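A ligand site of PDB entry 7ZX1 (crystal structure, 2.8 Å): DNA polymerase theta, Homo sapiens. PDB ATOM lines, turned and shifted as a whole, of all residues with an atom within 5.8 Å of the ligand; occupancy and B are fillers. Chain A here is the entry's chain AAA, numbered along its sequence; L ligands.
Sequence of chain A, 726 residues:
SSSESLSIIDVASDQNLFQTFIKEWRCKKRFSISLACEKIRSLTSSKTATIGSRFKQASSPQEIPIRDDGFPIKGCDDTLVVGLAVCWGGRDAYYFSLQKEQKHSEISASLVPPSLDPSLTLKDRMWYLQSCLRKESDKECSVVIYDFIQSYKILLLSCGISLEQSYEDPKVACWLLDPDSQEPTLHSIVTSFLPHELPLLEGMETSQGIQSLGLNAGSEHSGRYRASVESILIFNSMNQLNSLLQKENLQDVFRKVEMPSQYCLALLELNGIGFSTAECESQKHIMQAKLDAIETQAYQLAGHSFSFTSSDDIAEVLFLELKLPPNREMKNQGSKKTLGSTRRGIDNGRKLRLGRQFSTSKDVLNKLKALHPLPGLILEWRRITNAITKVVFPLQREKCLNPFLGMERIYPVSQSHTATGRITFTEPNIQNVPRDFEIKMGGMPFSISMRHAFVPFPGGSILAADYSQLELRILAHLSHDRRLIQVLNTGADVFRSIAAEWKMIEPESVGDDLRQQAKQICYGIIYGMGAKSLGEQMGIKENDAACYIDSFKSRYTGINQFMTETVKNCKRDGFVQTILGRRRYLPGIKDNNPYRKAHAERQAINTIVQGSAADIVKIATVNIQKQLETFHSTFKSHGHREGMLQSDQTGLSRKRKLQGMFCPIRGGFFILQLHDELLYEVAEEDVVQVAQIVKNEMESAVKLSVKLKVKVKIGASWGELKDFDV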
ATOM      1  N   LEU A 472      -8.790 -13.819  28.387  1.00  0.00           N
ATOM      2  CA  LEU A 472      -8.519 -15.040  29.186  1.00  0.00           C
ATOM      3  C   LEU A 472      -8.819 -14.760  30.656  1.00  0.00           C
ATOM      4  O   LEU A 472      -9.346 -15.658  31.353  1.00  0.00           O
ATOM      5  CB  LEU A 472      -7.068 -15.470  29.004  1.00  0.00           C
ATOM      6  CG  LEU A 472      -6.692 -16.011  27.619  1.00  0.00           C
ATOM      7  CD1 LEU A 472      -5.244 -16.468  27.628  1.00  0.00           C
ATOM      8  CD2 LEU A 472      -7.619 -17.165  27.195  1.00  0.00           C
ATOM      9  N   LEU A 484      -6.899 -22.542  34.686  1.00  0.00           N
ATOM     10  CA  LEU A 484      -6.587 -21.311  33.884  1.00  0.00           C
ATOM     11  C   LEU A 484      -6.046 -20.228  34.844  1.00  0.00           C
ATOM     12  O   LEU A 484      -5.084 -19.579  34.456  1.00  0.00           O
ATOM     13  CB  LEU A 484      -7.866 -20.850  33.164  1.00  0.00           C
ATOM     14  CG  LEU A 484      -7.766 -19.543  32.371  1.00  0.00           C
ATOM     15  CD1 LEU A 484      -6.509 -19.515  31.508  1.00  0.00           C
ATOM     16  CD2 LEU A 484      -8.993 -19.383  31.493  1.00  0.00           C
ATOM     17  N   VAL A 487      -2.306 -21.039  35.595  1.00  0.00           N
ATOM     18  CA  VAL A 487      -1.525 -20.680  34.368  1.00  0.00           C
ATOM     19  C   VAL A 487      -1.288 -19.155  34.380  1.00  0.00           C
ATOM     20  O   VAL A 487      -0.120 -18.723  34.228  1.00  0.00           O
ATOM     21  CB  VAL A 487      -2.276 -21.077  33.082  1.00  0.00           C
ATOM     22  CG1 VAL A 487      -1.569 -20.549  31.844  1.00  0.00           C
ATOM     23  CG2 VAL A 487      -2.510 -22.578  32.970  1.00  0.00           C
ATOM     24  N   VAL A 494       1.499 -18.479  27.120  1.00  0.00           N
ATOM     25  CA  VAL A 494       0.654 -19.643  26.732  1.00  0.00           C
ATOM     26  C   VAL A 494       0.849 -19.897  25.231  1.00  0.00           C
ATOM     27  O   VAL A 494       0.935 -21.067  24.810  1.00  0.00           O
ATOM     28  CB  VAL A 494      -0.825 -19.429  27.064  1.00  0.00           C
ATOM     29  CG1 VAL A 494      -1.660 -20.607  26.614  1.00  0.00           C
ATOM     30  CG2 VAL A 494      -1.055 -19.167  28.545  1.00  0.00           C
ATOM     31  N   SER A 497       4.172 -21.670  24.671  1.00  0.00           N
ATOM     32  CA  SER A 497       3.988 -23.043  25.205  1.00  0.00           C
ATOM     33  C   SER A 497       3.319 -23.908  24.118  1.00  0.00           C
ATOM     34  O   SER A 497       3.827 -24.978  23.802  1.00  0.00           O
ATOM     35  CB  SER A 497       3.172 -23.065  26.477  1.00  0.00           C
ATOM     36  OG  SER A 497       3.720 -22.195  27.455  1.00  0.00           O
ATOM     37  N   ILE A 498       2.217 -23.432  23.531  1.00  0.00           N
ATOM     38  CA  ILE A 498       1.442 -24.176  22.490  1.00  0.00           C
ATOM     39  C   ILE A 498       2.356 -24.376  21.274  1.00  0.00           C
ATOM     40  O   ILE A 498       2.472 -25.538  20.764  1.00  0.00           O
ATOM     41  CB  ILE A 498       0.146 -23.430  22.129  1.00  0.00           C
ATOM     42  CG1 ILE A 498      -0.853 -23.458  23.289  1.00  0.00           C
ATOM     43  CG2 ILE A 498      -0.467 -23.961  20.826  1.00  0.00           C
ATOM     44  CD1 ILE A 498      -1.977 -22.439  23.172  1.00  0.00           C
ATOM     45  N   ALA A 499       3.001 -23.297  20.809  1.00  0.00           N
ATOM     46  CA  ALA A 499       3.901 -23.321  19.624  1.00  0.00           C
ATOM     47  C   ALA A 499       5.027 -24.343  19.831  1.00  0.00           C
ATOM     48  O   ALA A 499       5.330 -25.070  18.885  1.00  0.00           O
ATOM     49  CB  ALA A 499       4.476 -21.946  19.371  1.00  0.00           C
ATOM     50  N   GLU A 501       5.148 -27.063  21.947  1.00  0.00           N
ATOM     51  CA  GLU A 501       4.572 -28.430  22.017  1.00  0.00           C
ATOM     52  C   GLU A 501       4.305 -28.854  20.581  1.00  0.00           C
ATOM     53  O   GLU A 501       4.383 -30.028  20.368  1.00  0.00           O
ATOM     54  CB  GLU A 501       3.369 -28.452  22.971  1.00  0.00           C
ATOM     55  CG  GLU A 501       2.654 -29.781  23.020  1.00  0.00           C
ATOM     56  CD  GLU A 501       1.608 -29.913  24.118  1.00  0.00           C
ATOM     57  OE1 GLU A 501       0.685 -30.750  23.967  1.00  0.00           O
ATOM     58  OE2 GLU A 501       1.722 -29.182  25.143  1.00  0.00           O
ATOM     59  N   TRP A 502       3.799 -27.939  19.753  1.00  0.00           N
ATOM     60  CA  TRP A 502       3.317 -28.211  18.374  1.00  0.00           C
ATOM     61  C   TRP A 502       4.539 -28.465  17.458  1.00  0.00           C
ATOM     62  O   TRP A 502       4.537 -29.483  16.752  1.00  0.00           O
ATOM     63  CB  TRP A 502       2.441 -27.030  17.919  1.00  0.00           C
ATOM     64  CG  TRP A 502       2.054 -27.060  16.477  1.00  0.00           C
ATOM     65  CD1 TRP A 502       1.825 -28.159  15.715  1.00  0.00           C
ATOM     66  CD2 TRP A 502       1.806 -25.925  15.630  1.00  0.00           C
ATOM     67  NE1 TRP A 502       1.523 -27.804  14.441  1.00  0.00           N
ATOM     68  CE2 TRP A 502       1.512 -26.435  14.355  1.00  0.00           C
ATOM     69  CE3 TRP A 502       1.832 -24.542  15.809  1.00  0.00           C
ATOM     70  CZ2 TRP A 502       1.188 -25.615  13.263  1.00  0.00           C
ATOM     71  CZ3 TRP A 502       1.567 -23.718  14.730  1.00  0.00           C
ATOM     72  CH2 TRP A 502       1.243 -24.252  13.478  1.00  0.00           C
ATOM     73  N   ILE A 521      -4.784 -20.426  17.188  1.00  0.00           N
ATOM     74  CA  ILE A 521      -5.130 -21.810  17.639  1.00  0.00           C
ATOM     75  C   ILE A 521      -5.807 -21.739  19.012  1.00  0.00           C
ATOM     76  O   ILE A 521      -6.847 -22.392  19.194  1.00  0.00           O
ATOM     77  CB  ILE A 521      -3.865 -22.689  17.639  1.00  0.00           C
ATOM     78  CG1 ILE A 521      -3.247 -22.830  16.241  1.00  0.00           C
ATOM     79  CG2 ILE A 521      -4.123 -24.045  18.266  1.00  0.00           C
ATOM     80  N   CYS A 522      -5.231 -21.012  19.951  1.00  0.00           N
ATOM     81  CA  CYS A 522      -5.689 -20.961  21.364  1.00  0.00           C
ATOM     82  C   CYS A 522      -7.056 -20.292  21.450  1.00  0.00           C
ATOM     83  O   CYS A 522      -7.966 -20.887  22.035  1.00  0.00           O
ATOM     84  CB  CYS A 522      -4.690 -20.192  22.213  1.00  0.00           C
ATOM     85  SG  CYS A 522      -5.191 -20.093  23.943  1.00  0.00           S
ATOM     86  N   ILE A 525      -9.795 -22.443  19.432  1.00  0.00           N
ATOM     87  CA  ILE A 525     -10.283 -23.622  20.198  1.00  0.00           C
ATOM     88  C   ILE A 525     -11.281 -23.094  21.233  1.00  0.00           C
ATOM     89  O   ILE A 525     -12.393 -23.629  21.268  1.00  0.00           O
ATOM     90  CB  ILE A 525      -9.108 -24.404  20.846  1.00  0.00           C
ATOM     91  CG1 ILE A 525      -8.191 -25.109  19.839  1.00  0.00           C
ATOM     92  CG2 ILE A 525      -9.613 -25.384  21.901  1.00  0.00           C
ATOM     93  N   ILE A 526     -10.908 -22.088  22.026  1.00  0.00           N
ATOM     94  CA  ILE A 526     -11.750 -21.542  23.134  1.00  0.00           C
ATOM     95  C   ILE A 526     -13.102 -21.094  22.564  1.00  0.00           C
ATOM     96  O   ILE A 526     -14.095 -21.230  23.289  1.00  0.00           O
ATOM     97  CB  ILE A 526     -11.048 -20.373  23.849  1.00  0.00           C
ATOM     98  CG1 ILE A 526      -9.772 -20.796  24.585  1.00  0.00           C
ATOM     99  CG2 ILE A 526     -12.026 -19.711  24.811  1.00  0.00           C
ATOM    100  CD1 ILE A 526      -8.892 -19.615  25.027  1.00  0.00           C
ATOM    101  N   LEU A 534      -9.064 -26.830  12.674  1.00  0.00           N
ATOM    102  CA  LEU A 534      -7.850 -26.839  13.548  1.00  0.00           C
ATOM    103  C   LEU A 534      -6.758 -27.639  12.825  1.00  0.00           C
ATOM    104  O   LEU A 534      -5.557 -27.210  12.857  1.00  0.00           O
ATOM    105  CB  LEU A 534      -8.238 -27.466  14.893  1.00  0.00           C
ATOM    106  CG  LEU A 534      -7.112 -27.579  15.918  1.00  0.00           C
ATOM    107  CD1 LEU A 534      -6.370 -26.261  16.099  1.00  0.00           C
ATOM    108  CD2 LEU A 534      -7.687 -28.029  17.243  1.00  0.00           C
ATOM    109  N   MET A 538      -3.016 -26.342  12.109  1.00  0.00           N
ATOM    110  CA  MET A 538      -1.908 -27.027  12.812  1.00  0.00           C
ATOM    111  C   MET A 538      -1.158 -27.965  11.835  1.00  0.00           C
ATOM    112  O   MET A 538      -0.056 -28.435  12.174  1.00  0.00           O
ATOM    113  CB  MET A 538      -2.425 -27.879  13.980  1.00  0.00           C
ATOM    114  CG  MET A 538      -2.786 -27.083  15.227  1.00  0.00           C
ATOM    115  SD  MET A 538      -3.009 -28.138  16.688  1.00  0.00           S
ATOM    116  CE  MET A 538      -1.305 -28.566  17.004  1.00  0.00           C
ATOM    117  N   TYR A 548      -6.853 -33.073  20.313  1.00  0.00           N
ATOM    118  CA  TYR A 548      -6.362 -31.800  20.913  1.00  0.00           C
ATOM    119  C   TYR A 548      -7.552 -31.067  21.545  1.00  0.00           C
ATOM    120  O   TYR A 548      -7.477 -30.656  22.738  1.00  0.00           O
ATOM    121  CB  TYR A 548      -5.667 -30.872  19.914  1.00  0.00           C
ATOM    122  CG  TYR A 548      -4.177 -31.090  19.797  1.00  0.00           C
ATOM    123  CD1 TYR A 548      -3.340 -30.838  20.877  1.00  0.00           C
ATOM    124  CD2 TYR A 548      -3.606 -31.557  18.626  1.00  0.00           C
ATOM    125  CE1 TYR A 548      -1.976 -31.064  20.787  1.00  0.00           C
ATOM    126  CE2 TYR A 548      -2.255 -31.825  18.537  1.00  0.00           C
ATOM    127  CZ  TYR A 548      -1.422 -31.539  19.603  1.00  0.00           C
ATOM    128  OH  TYR A 548      -0.076 -31.751  19.505  1.00  0.00           O
ATOM    129  N   SER A 551      -8.640 -32.843  24.807  1.00  0.00           N
ATOM    130  CA  SER A 551      -7.609 -32.583  25.845  1.00  0.00           C
ATOM    131  C   SER A 551      -7.882 -31.233  26.463  1.00  0.00           C
ATOM    132  O   SER A 551      -7.916 -31.213  27.714  1.00  0.00           O
ATOM    133  CB  SER A 551      -6.213 -32.657  25.247  1.00  0.00           C
ATOM    134  OG  SER A 551      -5.216 -32.209  26.157  1.00  0.00           O
ATOM    135  N   PHE A 552      -8.094 -30.170  25.691  1.00  0.00           N
ATOM    136  CA  PHE A 552      -8.436 -28.809  26.172  1.00  0.00           C
ATOM    137  C   PHE A 552      -9.640 -28.866  27.124  1.00  0.00           C
ATOM    138  O   PHE A 552      -9.556 -28.437  28.294  1.00  0.00           O
ATOM    139  CB  PHE A 552      -8.702 -27.843  25.019  1.00  0.00           C
ATOM    140  CG  PHE A 552      -9.448 -26.593  25.433  1.00  0.00           C
ATOM    141  CD1 PHE A 552      -8.804 -25.573  26.112  1.00  0.00           C
ATOM    142  CD2 PHE A 552     -10.798 -26.442  25.132  1.00  0.00           C
ATOM    143  CE1 PHE A 552      -9.483 -24.420  26.473  1.00  0.00           C
ATOM    144  CE2 PHE A 552     -11.478 -25.289  25.492  1.00  0.00           C
ATOM    145  CZ  PHE A 552     -10.825 -24.283  26.176  1.00  0.00           C
ATOM    146  N   ARG A 555      -8.898 -30.700  30.472  1.00  0.00           N
ATOM    147  CA  ARG A 555      -7.956 -29.968  31.390  1.00  0.00           C
ATOM    148  C   ARG A 555      -8.645 -28.764  32.003  1.00  0.00           C
ATOM    149  O   ARG A 555      -8.406 -28.494  33.196  1.00  0.00           O
ATOM    150  CB  ARG A 555      -6.687 -29.550  30.634  1.00  0.00           C
ATOM    151  CG  ARG A 555      -5.916 -30.699  30.003  1.00  0.00           C
ATOM    152  CD  ARG A 555      -4.463 -30.337  29.753  1.00  0.00           C
ATOM    153  NE  ARG A 555      -3.947 -30.948  28.539  1.00  0.00           N
ATOM    154  CZ  ARG A 555      -2.695 -30.834  28.106  1.00  0.00           C
ATOM    155  NH1 ARG A 555      -1.794 -30.147  28.799  1.00  0.00           N
ATOM    156  NH2 ARG A 555      -2.333 -31.423  26.973  1.00  0.00           N
ATOM    157  N   TYR A 556      -9.538 -28.079  31.260  1.00  0.00           N
ATOM    158  CA  TYR A 556     -10.223 -26.851  31.772  1.00  0.00           C
ATOM    159  C   TYR A 556     -11.740 -27.092  31.788  1.00  0.00           C
ATOM    160  O   TYR A 556     -12.425 -26.629  30.875  1.00  0.00           O
ATOM    161  CB  TYR A 556      -9.842 -25.631  30.920  1.00  0.00           C
ATOM    162  CG  TYR A 556      -8.373 -25.568  30.621  1.00  0.00           C
ATOM    163  CD1 TYR A 556      -7.509 -24.988  31.535  1.00  0.00           C
ATOM    164  CD2 TYR A 556      -7.830 -26.089  29.462  1.00  0.00           C
ATOM    165  CE1 TYR A 556      -6.145 -24.904  31.295  1.00  0.00           C
ATOM    166  CE2 TYR A 556      -6.481 -26.042  29.200  1.00  0.00           C
ATOM    167  CZ  TYR A 556      -5.620 -25.446  30.126  1.00  0.00           C
ATOM    168  OH  TYR A 556      -4.279 -25.380  29.889  1.00  0.00           O
ATOM    169  N   ILE A 559     -14.312 -23.976  32.257  1.00  0.00           N
ATOM    170  CA  ILE A 559     -14.578 -23.260  30.981  1.00  0.00           C
ATOM    171  C   ILE A 559     -15.754 -23.954  30.288  1.00  0.00           C
ATOM    172  O   ILE A 559     -16.717 -23.247  29.939  1.00  0.00           O
ATOM    173  CB  ILE A 559     -13.321 -23.178  30.096  1.00  0.00           C
ATOM    174  CG1 ILE A 559     -12.247 -22.282  30.742  1.00  0.00           C
ATOM    175  CG2 ILE A 559     -13.679 -22.699  28.689  1.00  0.00           C
ATOM    176  CD1 ILE A 559     -10.935 -22.230  30.000  1.00  0.00           C
HETATM  177  C1  LIG L   1      -1.170 -24.532  26.670  1.00  0.00           C
HETATM  178  C2  LIG L   1      -2.331 -27.385  20.556  1.00  0.00           C
HETATM  179  C3  LIG L   1      -0.469 -25.834  27.001  1.00  0.00           C
HETATM  180  C4  LIG L   1      -0.714 -26.673  25.759  1.00  0.00           C
HETATM  181  C5  LIG L   1      -1.871 -27.986  22.828  1.00  0.00           C
HETATM  182  C6  LIG L   1      -2.109 -26.243  25.253  1.00  0.00           C
HETATM  183  C7  LIG L   1      -3.181 -27.298  25.511  1.00  0.00           C
HETATM  184  C8  LIG L   1      -4.718 -28.951  24.616  1.00  0.00           C
HETATM  185  C9  LIG L   1      -3.217 -27.767  23.173  1.00  0.00           C
HETATM  186  C10 LIG L   1      -1.416 -27.797  21.515  1.00  0.00           C
HETATM  187  C11 LIG L   1       0.032 -28.037  21.177  1.00  0.00           C
HETATM  188  N1  LIG L   1      -4.384 -24.593  24.924  1.00  0.00           N
HETATM  189  N2  LIG L   1      -2.368 -24.988  25.973  1.00  0.00           N
HETATM  190  C12 LIG L   1      -3.580 -24.363  25.974  1.00  0.00           C
HETATM  191  N3  LIG L   1      -3.646 -27.957  24.441  1.00  0.00           N
HETATM  192  C13 LIG L   1      -6.419 -24.406  23.659  1.00  0.00           C
HETATM  193  C14 LIG L   1      -5.611 -24.052  24.865  1.00  0.00           C
HETATM  194  O1  LIG L   1      -0.693 -28.061  26.063  1.00  0.00           O
HETATM  195  C15 LIG L   1      -3.657 -27.157  20.876  1.00  0.00           C
HETATM  196  C16 LIG L   1      -4.105 -27.342  22.168  1.00  0.00           C
HETATM  197  O2  LIG L   1      -3.633 -27.493  26.660  1.00  0.00           O
HETATM  198  C17 LIG L   1      -4.023 -23.498  27.034  1.00  0.00           C
HETATM  199  C18 LIG L   1      -3.181 -23.219  28.164  1.00  0.00           C
HETATM  200  N4  LIG L   1      -2.591 -23.087  29.148  1.00  0.00           N
HETATM  201  C19 LIG L   1      -5.306 -22.919  26.957  1.00  0.00           C
HETATM  202  C20 LIG L   1      -5.802 -21.983  28.027  1.00  0.00           C
HETATM  203  F1  LIG L   1      -5.638 -22.460  29.257  1.00  0.00           F
HETATM  204  F2  LIG L   1      -7.121 -21.697  27.928  1.00  0.00           F
HETATM  205  F3  LIG L   1      -5.127 -20.825  28.012  1.00  0.00           F
HETATM  206  C21 LIG L   1      -6.092 -23.213  25.848  1.00  0.00           C
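The side-chain hydroxyl of Ser 551 is in hydrogen-bond range of the guanidinium group of Arg 555 (3.0 Å).
NE1 of Trp 502 lies within hydrogen-bond range of O of Met 538, 2.8 Å away.
Merely in contact with the ligand: Leu 484 (3.8 Å), Val 487 (3.8 Å), Val 494 (3.4 Å), Ile 498 (3.4 Å), Cys 522 (3.8 Å), Ile 525 (3.8 Å), Ile 526 (3.99 Å), Met 538 (3.9 Å), Tyr 548 (3.4 Å), Ser 551 (3.6 Å), Phe 552 (3.6 Å) and Arg 555 (3.6 Å).
Hydrophobic or aromatic side chains within 4 Å of the ligand: Leu 484, Val 487, Val 494, Ile 498, Ile 525, Ile 526, Met 538, Tyr 548, Phe 552 and Tyr 556.
14 residues have an atom within 4 Å of the ligand: Leu 484, Val 487, Val 494, Ile 498, Glu 501, Cys 522, Ile 525, Ile 526, Met 538, Tyr 548, Ser 551, Phe 552, Arg 555 and Tyr 556.
The nearest printed residue that does not touch the ligand is Trp 502 (4.03 Å).
The side-chain hydroxyl (OH) of Tyr 556 sits at hydrogen-bond distance from a nitrogen (N4) of the ligand, at 2.9 Å.
The side-chain carboxylate (OE2) of Glu 501 lies within hydrogen-bond range of an oxygen (O1) of the ligand, 2.8 Å away.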
